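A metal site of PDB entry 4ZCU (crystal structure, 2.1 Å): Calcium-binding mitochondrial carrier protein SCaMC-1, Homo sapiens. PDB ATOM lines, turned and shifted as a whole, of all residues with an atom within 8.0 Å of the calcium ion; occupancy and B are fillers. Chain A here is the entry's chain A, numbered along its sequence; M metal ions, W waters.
N of Glu 34 lies within hydrogen-bond range of OD1 of Asp 31.
The side-chain carboxylate (OD2) of Asp 23 lies within hydrogen-bond range of the backbone NH (N) of Gly 28, at 3.0 Å.
The side-chain carboxylate of Asp 23 sits close to the backbone NH of Gly 26 (3.2 Å).
The side-chain carboxylate of Glu 34 lies close to the backbone NH of Arg 24, 3.3 Å away.
Water W1 lies within hydrogen-bond range of OD2 of Asp 27 (2.7 Å), OD2 of Asp 31 (2.8 Å) and ND2 of Asn 25 (3.3 Å).
Of the 16 residues printed, 5 come within 4 Å of the calcium ion.
O of Val 29 is bound to the calcium ion, at 2.3 Å.
The calcium ion is bound by OD1 of Asn 25.
OD1 of Asp 27 binds the calcium ion (2.3 Å).
The calcium ion is bound by the side-chain carboxylate (OE1) of Glu 34, 2.3 Å away.
OD1 of Asp 23 binds the calcium ion (2.3 Å).
Water W1 is bound to the calcium ion, 2.4 Å away.
OE2 of Glu 34 binds the calcium ion, at 2.4 Å.
The calcium ion has seven donor atoms within binding distance.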
ATOM      1  N   PHE A  19     -33.162  21.234  -7.195  1.00  0.00           N
ATOM      2  CA  PHE A  19     -32.089  21.018  -8.166  1.00  0.00           C
ATOM      3  C   PHE A  19     -32.418  19.889  -9.137  1.00  0.00           C
ATOM      4  O   PHE A  19     -32.201  20.029 -10.344  1.00  0.00           O
ATOM      5  CB  PHE A  19     -30.786  20.698  -7.438  1.00  0.00           C
ATOM      6  CG  PHE A  19     -29.592  20.640  -8.343  1.00  0.00           C
ATOM      7  CD1 PHE A  19     -28.906  21.793  -8.684  1.00  0.00           C
ATOM      8  CD2 PHE A  19     -29.143  19.426  -8.852  1.00  0.00           C
ATOM      9  CE1 PHE A  19     -27.803  21.747  -9.519  1.00  0.00           C
ATOM     10  CE2 PHE A  19     -28.045  19.374  -9.681  1.00  0.00           C
ATOM     11  CZ  PHE A  19     -27.376  20.529 -10.019  1.00  0.00           C
ATOM     12  N   LEU A  22     -34.830  21.226 -11.595  1.00  0.00           N
ATOM     13  CA  LEU A  22     -34.269  22.154 -12.577  1.00  0.00           C
ATOM     14  C   LEU A  22     -33.330  21.488 -13.575  1.00  0.00           C
ATOM     15  O   LEU A  22     -33.332  21.839 -14.756  1.00  0.00           O
ATOM     16  CB  LEU A  22     -33.532  23.289 -11.849  1.00  0.00           C
ATOM     17  CG  LEU A  22     -34.419  24.170 -10.962  1.00  0.00           C
ATOM     18  CD1 LEU A  22     -33.640  25.352 -10.403  1.00  0.00           C
ATOM     19  CD2 LEU A  22     -35.650  24.633 -11.717  1.00  0.00           C
ATOM     20  N   ASP A  23     -32.527  20.529 -13.118  1.00  0.00           N
ATOM     21  CA  ASP A  23     -31.568  19.865 -13.994  1.00  0.00           C
ATOM     22  C   ASP A  23     -32.280  18.865 -14.898  1.00  0.00           C
ATOM     23  O   ASP A  23     -32.425  17.689 -14.552  1.00  0.00           O
ATOM     24  CB  ASP A  23     -30.478  19.174 -13.180  1.00  0.00           C
ATOM     25  CG  ASP A  23     -29.409  18.546 -14.046  1.00  0.00           C
ATOM     26  OD1 ASP A  23     -29.250  18.971 -15.205  1.00  0.00           O
ATOM     27  OD2 ASP A  23     -28.717  17.623 -13.562  1.00  0.00           O
ATOM     28  N   ARG A  24     -32.718  19.339 -16.059  1.00  0.00           N
ATOM     29  CA  ARG A  24     -33.569  18.568 -16.964  1.00  0.00           C
ATOM     30  C   ARG A  24     -32.822  17.455 -17.692  1.00  0.00           C
ATOM     31  O   ARG A  24     -33.356  16.356 -17.871  1.00  0.00           O
ATOM     32  CB  ARG A  24     -34.231  19.502 -17.979  1.00  0.00           C
ATOM     33  CG  ARG A  24     -35.197  18.835 -18.944  1.00  0.00           C
ATOM     34  CD  ARG A  24     -35.770  19.855 -19.913  1.00  0.00           C
ATOM     35  NE  ARG A  24     -36.793  19.299 -20.797  1.00  0.00           N
ATOM     36  CZ  ARG A  24     -37.598  20.045 -21.562  1.00  0.00           C
ATOM     37  NH1 ARG A  24     -37.511  21.365 -21.521  1.00  0.00           N
ATOM     38  NH2 ARG A  24     -38.494  19.464 -22.348  1.00  0.00           N
ATOM     39  N   ASN A  25     -31.588  17.721 -18.101  1.00  0.00           N
ATOM     40  CA  ASN A  25     -30.809  16.737 -18.840  1.00  0.00           C
ATOM     41  C   ASN A  25     -29.978  15.855 -17.918  1.00  0.00           C
ATOM     42  O   ASN A  25     -29.311  14.927 -18.364  1.00  0.00           O
ATOM     43  CB  ASN A  25     -29.919  17.417 -19.873  1.00  0.00           C
ATOM     44  CG  ASN A  25     -28.831  18.269 -19.236  1.00  0.00           C
ATOM     45  OD1 ASN A  25     -28.895  18.591 -18.053  1.00  0.00           O
ATOM     46  ND2 ASN A  25     -27.827  18.638 -20.021  1.00  0.00           N
ATOM     47  N   GLY A  26     -30.024  16.155 -16.618  1.00  0.00           N
ATOM     48  CA  GLY A  26     -29.364  15.352 -15.610  1.00  0.00           C
ATOM     49  C   GLY A  26     -27.856  15.225 -15.748  1.00  0.00           C
ATOM     50  O   GLY A  26     -27.285  14.192 -15.414  1.00  0.00           O
ATOM     51  N   ASP A  27     -27.206  16.290 -16.228  1.00  0.00           N
ATOM     52  CA  ASP A  27     -25.756  16.265 -16.381  1.00  0.00           C
ATOM     53  C   ASP A  27     -25.031  16.800 -15.144  1.00  0.00           C
ATOM     54  O   ASP A  27     -23.814  16.977 -15.142  1.00  0.00           O
ATOM     55  CB  ASP A  27     -25.336  17.063 -17.616  1.00  0.00           C
ATOM     56  CG  ASP A  27     -25.709  18.532 -17.525  1.00  0.00           C
ATOM     57  OD1 ASP A  27     -26.552  18.878 -16.672  1.00  0.00           O
ATOM     58  OD2 ASP A  27     -25.160  19.329 -18.315  1.00  0.00           O
ATOM     59  N   GLY A  28     -25.798  17.061 -14.084  1.00  0.00           N
ATOM     60  CA  GLY A  28     -25.237  17.468 -12.808  1.00  0.00           C
ATOM     61  C   GLY A  28     -25.117  18.965 -12.608  1.00  0.00           C
ATOM     62  O   GLY A  28     -24.760  19.424 -11.518  1.00  0.00           O
ATOM     63  N   VAL A  29     -25.416  19.734 -13.646  1.00  0.00           N
ATOM     64  CA  VAL A  29     -25.382  21.186 -13.548  1.00  0.00           C
ATOM     65  C   VAL A  29     -26.661  21.798 -14.084  1.00  0.00           C
ATOM     66  O   VAL A  29     -27.374  21.182 -14.881  1.00  0.00           O
ATOM     67  CB  VAL A  29     -24.179  21.792 -14.309  1.00  0.00           C
ATOM     68  CG1 VAL A  29     -22.868  21.279 -13.719  1.00  0.00           C
ATOM     69  CG2 VAL A  29     -24.271  21.499 -15.790  1.00  0.00           C
ATOM     70  N   VAL A  30     -26.972  23.014 -13.640  1.00  0.00           N
ATOM     71  CA  VAL A  30     -28.084  23.762 -14.192  1.00  0.00           C
ATOM     72  C   VAL A  30     -27.563  24.966 -14.970  1.00  0.00           C
ATOM     73  O   VAL A  30     -26.886  25.828 -14.406  1.00  0.00           O
ATOM     74  CB  VAL A  30     -29.056  24.239 -13.093  1.00  0.00           C
ATOM     75  CG1 VAL A  30     -30.112  25.163 -13.692  1.00  0.00           C
ATOM     76  CG2 VAL A  30     -29.709  23.055 -12.406  1.00  0.00           C
ATOM     77  N   ASP A  31     -27.861  24.999 -16.256  1.00  0.00           N
ATOM     78  CA  ASP A  31     -27.496  26.150 -17.081  1.00  0.00           C
ATOM     79  C   ASP A  31     -28.640  27.160 -17.063  1.00  0.00           C
ATOM     80  O   ASP A  31     -29.705  26.878 -16.500  1.00  0.00           O
ATOM     81  CB  ASP A  31     -27.162  25.706 -18.507  1.00  0.00           C
ATOM     82  CG  ASP A  31     -28.221  24.804 -19.114  1.00  0.00           C
ATOM     83  OD1 ASP A  31     -29.420  25.150 -19.040  1.00  0.00           O
ATOM     84  OD2 ASP A  31     -27.851  23.745 -19.661  1.00  0.00           O
ATOM     85  N   ILE A  32     -28.422  28.318 -17.660  1.00  0.00           N
ATOM     86  CA  ILE A  32     -29.379  29.423 -17.553  1.00  0.00           C
ATOM     87  C   ILE A  32     -30.723  29.066 -18.193  1.00  0.00           C
ATOM     88  O   ILE A  32     -31.779  29.443 -17.682  1.00  0.00           O
ATOM     89  CB  ILE A  32     -28.815  30.718 -18.184  1.00  0.00           C
ATOM     90  CG1 ILE A  32     -29.806  31.869 -18.056  1.00  0.00           C
ATOM     91  CG2 ILE A  32     -28.401  30.493 -19.636  1.00  0.00           C
ATOM     92  CD1 ILE A  32     -30.165  32.199 -16.616  1.00  0.00           C
ATOM     93  N   GLU A  34     -32.043  26.059 -18.391  1.00  0.00           N
ATOM     94  CA  GLU A  34     -32.698  25.141 -17.464  1.00  0.00           C
ATOM     95  C   GLU A  34     -33.286  25.870 -16.269  1.00  0.00           C
ATOM     96  O   GLU A  34     -34.318  25.473 -15.735  1.00  0.00           O
ATOM     97  CB  GLU A  34     -31.714  24.077 -16.983  1.00  0.00           C
ATOM     98  CG  GLU A  34     -31.462  22.945 -17.978  1.00  0.00           C
ATOM     99  CD  GLU A  34     -30.387  21.994 -17.503  1.00  0.00           C
ATOM    100  OE1 GLU A  34     -29.506  22.430 -16.733  1.00  0.00           O
ATOM    101  OE2 GLU A  34     -30.421  20.809 -17.876  1.00  0.00           O
ATOM    102  N   LEU A  35     -32.624  26.933 -15.820  1.00  0.00           N
ATOM    103  CA  LEU A  35     -33.135  27.729 -14.705  1.00  0.00           C
ATOM    104  C   LEU A  35     -34.385  28.500 -15.114  1.00  0.00           C
ATOM    105  O   LEU A  35     -35.360  28.554 -14.378  1.00  0.00           O
ATOM    106  CB  LEU A  35     -32.058  28.691 -14.189  1.00  0.00           C
ATOM    107  CG  LEU A  35     -32.515  29.636 -13.069  1.00  0.00           C
ATOM    108  CD1 LEU A  35     -32.940  28.859 -11.836  1.00  0.00           C
ATOM    109  CD2 LEU A  35     -31.411  30.627 -12.731  1.00  0.00           C
ATOM    110  N   LYS A  65     -22.039  27.826 -14.940  1.00  0.00           N
ATOM    111  CA  LYS A  65     -22.856  26.673 -14.572  1.00  0.00           C
ATOM    112  C   LYS A  65     -23.106  26.622 -13.074  1.00  0.00           C
ATOM    113  O   LYS A  65     -22.244  26.992 -12.280  1.00  0.00           O
ATOM    114  CB  LYS A  65     -22.160  25.380 -15.014  1.00  0.00           C
ATOM    115  CG  LYS A  65     -22.163  25.117 -16.505  1.00  0.00           C
ATOM    116  CD  LYS A  65     -21.263  23.934 -16.835  1.00  0.00           C
ATOM    117  CE  LYS A  65     -19.829  24.199 -16.399  1.00  0.00           C
ATOM    118  NZ  LYS A  65     -18.904  23.103 -16.777  1.00  0.00           N
ATOM    119  N   LEU A  66     -24.300  26.174 -12.694  1.00  0.00           N
ATOM    120  CA  LEU A  66     -24.603  25.964 -11.283  1.00  0.00           C
ATOM    121  C   LEU A  66     -24.574  24.470 -10.974  1.00  0.00           C
ATOM    122  O   LEU A  66     -25.453  23.729 -11.404  1.00  0.00           O
ATOM    123  CB  LEU A  66     -25.969  26.534 -10.910  1.00  0.00           C
ATOM    124  CG  LEU A  66     -26.182  28.056 -10.976  1.00  0.00           C
ATOM    125  CD1 LEU A  66     -27.628  28.398 -10.674  1.00  0.00           C
ATOM    126  CD2 LEU A  66     -25.252  28.771 -10.004  1.00  0.00           C
HETATM  127 CA    CA M   1     -28.298  20.422 -16.788  1.00  0.00          CA
HETATM  128  O   HOH W   1     -26.915  21.422 -18.462  1.00  0.00           O
